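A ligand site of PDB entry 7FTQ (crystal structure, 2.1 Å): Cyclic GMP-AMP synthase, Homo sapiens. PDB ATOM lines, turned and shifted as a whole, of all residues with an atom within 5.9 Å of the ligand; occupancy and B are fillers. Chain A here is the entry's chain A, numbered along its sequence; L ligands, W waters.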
ATOM      1  N   LYS A  59      20.996   7.590   0.173  1.00  0.00           N
ATOM      2  CA  LYS A  59      21.011   6.129  -0.013  1.00  0.00           C
ATOM      3  C   LYS A  59      21.239   5.776  -1.516  1.00  0.00           C
ATOM      4  O   LYS A  59      20.536   6.306  -2.377  1.00  0.00           O
ATOM      5  CB  LYS A  59      19.690   5.504   0.501  1.00  0.00           C
ATOM      6  CG  LYS A  59      19.823   4.107   1.115  1.00  0.00           C
ATOM      7  CD  LYS A  59      18.542   3.633   1.826  1.00  0.00           C
ATOM      8  CE  LYS A  59      18.783   2.520   2.846  1.00  0.00           C
ATOM      9  NZ  LYS A  59      17.506   1.909   3.384  1.00  0.00           N
ATOM     10  N   LEU A 178      10.277  -8.739  10.985  1.00  0.00           N
ATOM     11  CA  LEU A 178      11.572  -8.406  11.592  1.00  0.00           C
ATOM     12  C   LEU A 178      12.051  -9.606  12.479  1.00  0.00           C
ATOM     13  O   LEU A 178      12.338  -9.456  13.674  1.00  0.00           O
ATOM     14  CB  LEU A 178      11.495  -7.049  12.366  1.00  0.00           C
ATOM     15  CG  LEU A 178      12.852  -6.439  12.844  1.00  0.00           C
ATOM     16  CD1 LEU A 178      13.744  -6.005  11.661  1.00  0.00           C
ATOM     17  CD2 LEU A 178      12.638  -5.307  13.841  1.00  0.00           C
ATOM     18  N   ILE A 180      14.447 -11.322  13.676  1.00  0.00           N
ATOM     19  CA  ILE A 180      15.878 -11.232  13.972  1.00  0.00           C
ATOM     20  C   ILE A 180      16.231 -11.839  15.331  1.00  0.00           C
ATOM     21  O   ILE A 180      17.405 -11.812  15.697  1.00  0.00           O
ATOM     22  CB  ILE A 180      16.348  -9.736  13.886  1.00  0.00           C
ATOM     23  CG1 ILE A 180      15.661  -8.853  14.972  1.00  0.00           C
ATOM     24  CG2 ILE A 180      16.177  -9.148  12.443  1.00  0.00           C
ATOM     25  CD1 ILE A 180      16.068  -7.466  14.998  1.00  0.00           C
ATOM     26  N   TRP A 183      19.085 -14.190  15.706  1.00  0.00           N
ATOM     27  CA  TRP A 183      20.271 -13.606  15.092  1.00  0.00           C
ATOM     28  C   TRP A 183      20.760 -12.414  15.902  1.00  0.00           C
ATOM     29  O   TRP A 183      21.815 -12.512  16.555  1.00  0.00           O
ATOM     30  CB  TRP A 183      19.970 -13.265  13.616  1.00  0.00           C
ATOM     31  CG  TRP A 183      20.950 -12.344  12.945  1.00  0.00           C
ATOM     32  CD1 TRP A 183      22.298 -12.209  13.209  1.00  0.00           C
ATOM     33  CD2 TRP A 183      20.655 -11.417  11.885  1.00  0.00           C
ATOM     34  NE1 TRP A 183      22.851 -11.282  12.356  1.00  0.00           N
ATOM     35  CE2 TRP A 183      21.855 -10.731  11.570  1.00  0.00           C
ATOM     36  CE3 TRP A 183      19.463 -11.026  11.238  1.00  0.00           C
ATOM     37  CZ2 TRP A 183      21.904  -9.690  10.631  1.00  0.00           C
ATOM     38  CZ3 TRP A 183      19.511  -9.997  10.292  1.00  0.00           C
ATOM     39  CH2 TRP A 183      20.731  -9.370   9.974  1.00  0.00           C
ATOM     40  N   ARG A 216       1.881   3.420   1.901  1.00  0.00           N
ATOM     41  CA  ARG A 216       2.609   2.186   2.148  1.00  0.00           C
ATOM     42  C   ARG A 216       3.524   2.339   3.404  1.00  0.00           C
ATOM     43  O   ARG A 216       4.124   3.396   3.574  1.00  0.00           O
ATOM     44  CB  ARG A 216       3.428   1.818   0.894  1.00  0.00           C
ATOM     45  CG  ARG A 216       4.214   0.494   0.963  1.00  0.00           C
ATOM     46  CD  ARG A 216       5.317   0.385  -0.082  1.00  0.00           C
ATOM     47  NE  ARG A 216       6.416   1.341   0.124  1.00  0.00           N
ATOM     48  CZ  ARG A 216       7.498   1.110   0.871  1.00  0.00           C
ATOM     49  NH1 ARG A 216       7.654  -0.047   1.494  1.00  0.00           N
ATOM     50  NH2 ARG A 216       8.436   2.042   0.995  1.00  0.00           N
ATOM     51  N   LEU A 217       3.629   1.296   4.263  1.00  0.00           N
ATOM     52  CA  LEU A 217       4.513   1.329   5.435  1.00  0.00           C
ATOM     53  C   LEU A 217       5.949   1.279   4.924  1.00  0.00           C
ATOM     54  O   LEU A 217       6.225   0.577   3.942  1.00  0.00           O
ATOM     55  CB  LEU A 217       4.294   0.132   6.374  1.00  0.00           C
ATOM     56  CG  LEU A 217       2.990   0.030   7.145  1.00  0.00           C
ATOM     57  CD1 LEU A 217       3.000  -1.217   8.017  1.00  0.00           C
ATOM     58  CD2 LEU A 217       2.779   1.220   8.044  1.00  0.00           C
ATOM     59  N   SER A 218       6.858   2.030   5.552  1.00  0.00           N
ATOM     60  CA  SER A 218       8.262   2.057   5.139  1.00  0.00           C
ATOM     61  C   SER A 218       9.155   1.913   6.356  1.00  0.00           C
ATOM     62  O   SER A 218       8.962   2.595   7.357  1.00  0.00           O
ATOM     63  CB  SER A 218       8.560   3.358   4.399  1.00  0.00           C
ATOM     64  OG  SER A 218       9.933   3.455   4.054  1.00  0.00           O
ATOM     65  N   PHE A 219      10.098   0.976   6.273  1.00  0.00           N
ATOM     66  CA  PHE A 219      11.038   0.686   7.341  1.00  0.00           C
ATOM     67  C   PHE A 219      12.489   0.810   6.839  1.00  0.00           C
ATOM     68  O   PHE A 219      13.422   0.236   7.425  1.00  0.00           O
ATOM     69  CB  PHE A 219      10.733  -0.690   7.930  1.00  0.00           C
ATOM     70  CG  PHE A 219       9.379  -0.813   8.578  1.00  0.00           C
ATOM     71  CD1 PHE A 219       9.179  -0.414   9.902  1.00  0.00           C
ATOM     72  CD2 PHE A 219       8.303  -1.355   7.880  1.00  0.00           C
ATOM     73  CE1 PHE A 219       7.924  -0.541  10.496  1.00  0.00           C
ATOM     74  CE2 PHE A 219       7.044  -1.461   8.482  1.00  0.00           C
ATOM     75  CZ  PHE A 219       6.860  -1.050   9.783  1.00  0.00           C
ATOM     76  N   SER A 220      12.680   1.629   5.802  1.00  0.00           N
ATOM     77  CA  SER A 220      13.974   1.902   5.178  1.00  0.00           C
ATOM     78  C   SER A 220      15.029   2.391   6.191  1.00  0.00           C
ATOM     79  O   SER A 220      16.204   2.045   6.073  1.00  0.00           O
ATOM     80  CB  SER A 220      13.794   2.931   4.065  1.00  0.00           C
ATOM     81  OG  SER A 220      15.044   3.222   3.460  1.00  0.00           O
ATOM     82  N   HIS A 221      14.607   3.190   7.176  1.00  0.00           N
ATOM     83  CA  HIS A 221      15.460   3.786   8.213  1.00  0.00           C
ATOM     84  C   HIS A 221      16.074   2.752   9.159  1.00  0.00           C
ATOM     85  O   HIS A 221      17.061   3.049   9.827  1.00  0.00           O
ATOM     86  CB  HIS A 221      14.659   4.838   8.980  1.00  0.00           C
ATOM     87  CG  HIS A 221      13.550   4.260   9.820  1.00  0.00           C
ATOM     88  ND1 HIS A 221      12.443   3.652   9.238  1.00  0.00           N
ATOM     89  CD2 HIS A 221      13.409   4.231  11.158  1.00  0.00           C
ATOM     90  CE1 HIS A 221      11.681   3.268  10.244  1.00  0.00           C
ATOM     91  NE2 HIS A 221      12.207   3.620  11.418  1.00  0.00           N
ATOM     92  N   ILE A 222      15.482   1.548   9.221  1.00  0.00           N
ATOM     93  CA  ILE A 222      15.961   0.472  10.066  1.00  0.00           C
ATOM     94  C   ILE A 222      17.206  -0.202   9.430  1.00  0.00           C
ATOM     95  O   ILE A 222      18.015  -0.772  10.157  1.00  0.00           O
ATOM     96  CB  ILE A 222      14.820  -0.528  10.454  1.00  0.00           C
ATOM     97  CG1 ILE A 222      13.565   0.174  11.086  1.00  0.00           C
ATOM     98  CG2 ILE A 222      15.309  -1.687  11.369  1.00  0.00           C
ATOM     99  CD1 ILE A 222      13.750   0.808  12.543  1.00  0.00           C
ATOM    100  N   GLU A 223      17.354  -0.157   8.092  1.00  0.00           N
ATOM    101  CA  GLU A 223      18.476  -0.783   7.383  1.00  0.00           C
ATOM    102  C   GLU A 223      19.829  -0.394   7.914  1.00  0.00           C
ATOM    103  O   GLU A 223      20.625  -1.281   8.218  1.00  0.00           O
ATOM    104  CB  GLU A 223      18.404  -0.542   5.866  1.00  0.00           C
ATOM    105  CG  GLU A 223      19.370  -1.466   5.119  1.00  0.00           C
ATOM    106  CD  GLU A 223      19.504  -1.239   3.630  1.00  0.00           C
ATOM    107  OE1 GLU A 223      18.581  -0.657   3.028  1.00  0.00           O
ATOM    108  OE2 GLU A 223      20.527  -1.678   3.057  1.00  0.00           O
ATOM    109  N   LYS A 224      20.105   0.899   8.051  1.00  0.00           N
ATOM    110  CA  LYS A 224      21.403   1.384   8.569  1.00  0.00           C
ATOM    111  C   LYS A 224      21.648   0.847   9.983  1.00  0.00           C
ATOM    112  O   LYS A 224      22.797   0.540  10.302  1.00  0.00           O
ATOM    113  CB  LYS A 224      21.510   2.921   8.508  1.00  0.00           C
ATOM    114  CG  LYS A 224      20.514   3.669   9.418  1.00  0.00           C
ATOM    115  CD  LYS A 224      20.564   5.190   9.257  1.00  0.00           C
ATOM    116  CE  LYS A 224      21.410   5.864  10.303  1.00  0.00           C
ATOM    117  NZ  LYS A 224      22.624   6.487   9.715  1.00  0.00           N
ATOM    118  N   ILE A 226      20.829  -2.088  11.189  1.00  0.00           N
ATOM    119  CA  ILE A 226      21.204  -3.498  11.144  1.00  0.00           C
ATOM    120  C   ILE A 226      22.435  -3.755  10.267  1.00  0.00           C
ATOM    121  O   ILE A 226      23.259  -4.582  10.647  1.00  0.00           O
ATOM    122  CB  ILE A 226      19.987  -4.331  10.711  1.00  0.00           C
ATOM    123  CG1 ILE A 226      18.975  -4.400  11.870  1.00  0.00           C
ATOM    124  CG2 ILE A 226      20.421  -5.726  10.239  1.00  0.00           C
ATOM    125  CD1 ILE A 226      17.607  -4.810  11.476  1.00  0.00           C
ATOM    126  N   TYR A 276      16.088  -3.423  -3.798  1.00  0.00           N
ATOM    127  CA  TYR A 276      15.188  -3.680  -2.661  1.00  0.00           C
ATOM    128  C   TYR A 276      14.826  -5.193  -2.537  1.00  0.00           C
ATOM    129  O   TYR A 276      14.807  -5.719  -1.428  1.00  0.00           O
ATOM    130  CB  TYR A 276      13.921  -2.803  -2.751  1.00  0.00           C
ATOM    131  CG  TYR A 276      12.902  -3.095  -1.672  1.00  0.00           C
ATOM    132  CD1 TYR A 276      13.224  -2.936  -0.317  1.00  0.00           C
ATOM    133  CD2 TYR A 276      11.622  -3.514  -1.998  1.00  0.00           C
ATOM    134  CE1 TYR A 276      12.286  -3.193   0.675  1.00  0.00           C
ATOM    135  CE2 TYR A 276      10.671  -3.766  -1.012  1.00  0.00           C
ATOM    136  CZ  TYR A 276      11.025  -3.634   0.325  1.00  0.00           C
ATOM    137  OH  TYR A 276      10.077  -3.906   1.289  1.00  0.00           O
ATOM    138  N   LYS A 279      18.139  -6.973  -1.276  1.00  0.00           N
ATOM    139  CA  LYS A 279      18.347  -6.692   0.158  1.00  0.00           C
ATOM    140  C   LYS A 279      17.385  -7.522   1.007  1.00  0.00           C
ATOM    141  O   LYS A 279      17.788  -8.046   2.049  1.00  0.00           O
ATOM    142  CB  LYS A 279      18.097  -5.218   0.519  1.00  0.00           C
ATOM    143  CG  LYS A 279      19.097  -4.190  -0.003  1.00  0.00           C
ATOM    144  CD  LYS A 279      18.552  -2.797   0.352  1.00  0.00           C
ATOM    145  CE  LYS A 279      19.415  -1.668  -0.132  1.00  0.00           C
ATOM    146  NZ  LYS A 279      18.660  -0.392  -0.112  1.00  0.00           N
ATOM    147  N   THR A 280      16.110  -7.609   0.594  1.00  0.00           N
ATOM    148  CA  THR A 280      15.108  -8.363   1.363  1.00  0.00           C
ATOM    149  C   THR A 280      15.539  -9.831   1.431  1.00  0.00           C
ATOM    150  O   THR A 280      15.524 -10.397   2.496  1.00  0.00           O
ATOM    151  CB  THR A 280      13.720  -8.193   0.718  1.00  0.00           C
ATOM    152  OG1 THR A 280      13.365  -6.808   0.790  1.00  0.00           O
ATOM    153  CG2 THR A 280      12.642  -9.073   1.422  1.00  0.00           C
ATOM    154  N   PHE A 283      18.618 -10.282   3.753  1.00  0.00           N
ATOM    155  CA  PHE A 283      18.209 -10.226   5.163  1.00  0.00           C
ATOM    156  C   PHE A 283      17.442 -11.476   5.571  1.00  0.00           C
ATOM    157  O   PHE A 283      17.685 -11.939   6.667  1.00  0.00           O
ATOM    158  CB  PHE A 283      17.502  -8.898   5.506  1.00  0.00           C
ATOM    159  CG  PHE A 283      18.471  -7.730   5.602  1.00  0.00           C
ATOM    160  CD1 PHE A 283      19.487  -7.725   6.560  1.00  0.00           C
ATOM    161  CD2 PHE A 283      18.409  -6.668   4.704  1.00  0.00           C
ATOM    162  CE1 PHE A 283      20.430  -6.665   6.622  1.00  0.00           C
ATOM    163  CE2 PHE A 283      19.336  -5.596   4.775  1.00  0.00           C
ATOM    164  CZ  PHE A 283      20.345  -5.619   5.726  1.00  0.00           C
ATOM    165  N   ASN A 322       7.940  -9.481   2.409  1.00  0.00           N
ATOM    166  CA  ASN A 322       8.524  -8.223   2.882  1.00  0.00           C
ATOM    167  C   ASN A 322       9.147  -8.565   4.274  1.00  0.00           C
ATOM    168  O   ASN A 322       8.512  -9.254   5.076  1.00  0.00           O
ATOM    169  CB  ASN A 322       7.395  -7.184   3.037  1.00  0.00           C
ATOM    170  CG  ASN A 322       7.798  -5.875   3.652  1.00  0.00           C
ATOM    171  OD1 ASN A 322       8.363  -5.802   4.759  1.00  0.00           O
ATOM    172  ND2 ASN A 322       7.437  -4.786   2.985  1.00  0.00           N
ATOM    173  N   TYR A 323      10.362  -8.101   4.565  1.00  0.00           N
ATOM    174  CA  TYR A 323      11.060  -8.409   5.829  1.00  0.00           C
ATOM    175  C   TYR A 323      10.290  -7.986   7.079  1.00  0.00           C
ATOM    176  O   TYR A 323      10.464  -8.573   8.130  1.00  0.00           O
ATOM    177  CB  TYR A 323      12.452  -7.737   5.849  1.00  0.00           C
ATOM    178  CG  TYR A 323      13.404  -8.459   6.779  1.00  0.00           C
ATOM    179  CD1 TYR A 323      13.823  -9.762   6.503  1.00  0.00           C
ATOM    180  CD2 TYR A 323      13.898  -7.840   7.925  1.00  0.00           C
ATOM    181  CE1 TYR A 323      14.636 -10.461   7.377  1.00  0.00           C
ATOM    182  CE2 TYR A 323      14.787  -8.514   8.785  1.00  0.00           C
ATOM    183  CZ  TYR A 323      15.163  -9.818   8.492  1.00  0.00           C
ATOM    184  OH  TYR A 323      16.035 -10.499   9.310  1.00  0.00           O
ATOM    185  N   PHE A 324       9.470  -6.930   6.966  1.00  0.00           N
ATOM    186  CA  PHE A 324       8.659  -6.414   8.080  1.00  0.00           C
ATOM    187  C   PHE A 324       7.195  -6.870   8.058  1.00  0.00           C
ATOM    188  O   PHE A 324       6.557  -6.867   9.086  1.00  0.00           O
ATOM    189  CB  PHE A 324       8.748  -4.881   8.057  1.00  0.00           C
ATOM    190  CG  PHE A 324      10.146  -4.392   8.315  1.00  0.00           C
ATOM    191  CD1 PHE A 324      11.089  -4.355   7.290  1.00  0.00           C
ATOM    192  CD2 PHE A 324      10.550  -4.044   9.601  1.00  0.00           C
ATOM    193  CE1 PHE A 324      12.407  -3.990   7.561  1.00  0.00           C
ATOM    194  CE2 PHE A 324      11.857  -3.625   9.853  1.00  0.00           C
ATOM    195  CZ  PHE A 324      12.777  -3.616   8.837  1.00  0.00           C
HETATM  196  C1  LIG L   1      12.999  -1.598   4.100  1.00  0.00           C
HETATM  197  C2  LIG L   1      10.999  -0.314   3.250  1.00  0.00           C
HETATM  198  O1  LIG L   1      10.298  -0.860   4.240  1.00  0.00           O
HETATM  199  C3  LIG L   1      13.260  -0.157   2.157  1.00  0.00           C
HETATM  200  C4  LIG L   1      14.606  -0.520   2.120  1.00  0.00           C
HETATM  201  C5  LIG L   1      14.121   0.837   0.469  1.00  0.00           C
HETATM  202  C6  LIG L   1      15.699  -5.076   5.758  1.00  0.00           C
HETATM  203  C7  LIG L   1      16.602  -5.521   8.063  1.00  0.00           C
HETATM  204  C8  LIG L   1      16.116  -4.585   6.995  1.00  0.00           C
HETATM  205  C9  LIG L   1      15.870  -3.241   7.239  1.00  0.00           C
HETATM  206  C10 LIG L   1      15.325  -2.389   6.311  1.00  0.00           C
HETATM  207  C11 LIG L   1      14.931  -2.865   5.071  1.00  0.00           C
HETATM  208  C12 LIG L   1      15.168  -4.225   4.799  1.00  0.00           C
HETATM  209  C13 LIG L   1      14.359  -1.917   4.069  1.00  0.00           C
HETATM  210  C14 LIG L   1      15.168  -1.384   3.053  1.00  0.00           C
HETATM  211  C15 LIG L   1      12.450  -0.702   3.166  1.00  0.00           C
HETATM  212  F1  LIG L   1      16.219  -2.754   8.441  1.00  0.00           F
HETATM  213  N1  LIG L   1      15.131   0.113   1.016  1.00  0.00           N
HETATM  214  N2  LIG L   1      12.971   0.725   1.117  1.00  0.00           N
HETATM  215  O2  LIG L   1      10.496   0.448   2.422  1.00  0.00           O
HETATM  216 CL1  LIG L   1      14.739  -4.899   3.260  1.00  0.00          CL
HETATM  217  O   HOH W   1       7.779  -2.038   4.110  1.00  0.00           O
HETATM  218  O   HOH W   2      10.500  -3.595   3.953  1.00  0.00           O
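NZ of Lys 279 is in salt-bridge range of OE1 of Glu 223.
The side-chain carboxylate (OE1) of Glu 223 lies within salt-bridge range of the side-chain amino group (NZ) of Lys 59, at 2.8 Å.
The backbone carbonyl oxygen of Phe 283 lies within hydrogen-bond range of the side-chain hydroxyl of Tyr 323.
The side-chain hydroxyl of Thr 280 is in hydrogen-bond range of the backbone carbonyl oxygen of Tyr 276 (2.9 Å).
N of Phe 324 lies within hydrogen-bond range of OD1 of Asn 322 (2.7 Å).
The side-chain hydroxyl (OH) of Tyr 276 is in hydrogen-bond range of the side-chain amide nitrogen (ND2) of Asn 322 (3.3 Å).
NZ of Lys 59 is in hydrogen-bond range of OG of Ser 220, at 2.8 Å.
The backbone NH (N) of Leu 178 sits at hydrogen-bond distance from the backbone carbonyl oxygen (O) of Tyr 323 (2.9 Å).
N of Phe 219 is in hydrogen-bond range of O1 of the ligand, at 2.7 Å.
NH2 of Arg 216 lies within salt-bridge range of O2 of the ligand, 3.0 Å away.
The side-chain hydroxyl of Ser 218 sits at hydrogen-bond distance from an oxygen (O2) of the ligand (3.5 Å).
Water W2 lies within hydrogen-bond range of OH of Tyr 276 (2.7 Å), O1 of the ligand (2.8 Å) and OD1 of Asn 322 (3.2 Å).
Water W1 lies within hydrogen-bond range of an oxygen (O1) of the ligand (2.8 Å), the side-chain amide nitrogen of Asn 322 (3.0 Å), the backbone carbonyl oxygen of Leu 217 (3.0 Å) and the guanidinium group of Arg 216 (3.3 Å).
The backbone carbonyl oxygen (O) of Ile 222 sits close to a fluorine (F1) of the ligand (3.2 Å).
N of Glu 223 lies close to F1 of the ligand (2.9 Å).
Lys 59 touches the ligand.
Ser 220 touches the ligand.
CD1 of Ile 226 touches C7 of the ligand, at 3.6 Å.
CE1 of Tyr 276 touches C3 of the ligand, 3.5 Å away.
NZ of Lys 279 touches N1 of the ligand, 3.7 Å away.
Thr 280 touches the ligand.
CD2 of Phe 283 touches C6 of the ligand, at 3.3 Å.
CD2 of Tyr 323 touches C7 of the ligand, at 3.6 Å.
Phe 324 touches the ligand.
Within 4 Å of the ligand: Lys 59, Arg 216, Ser 218, Phe 219, Ser 220, Ile 222, Glu 223, Ile 226, Tyr 276, Lys 279, Thr 280, Phe 283, Tyr 323 and Phe 324.
The nearest printed residue that does not touch the ligand is Leu 217 (4.3 Å).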
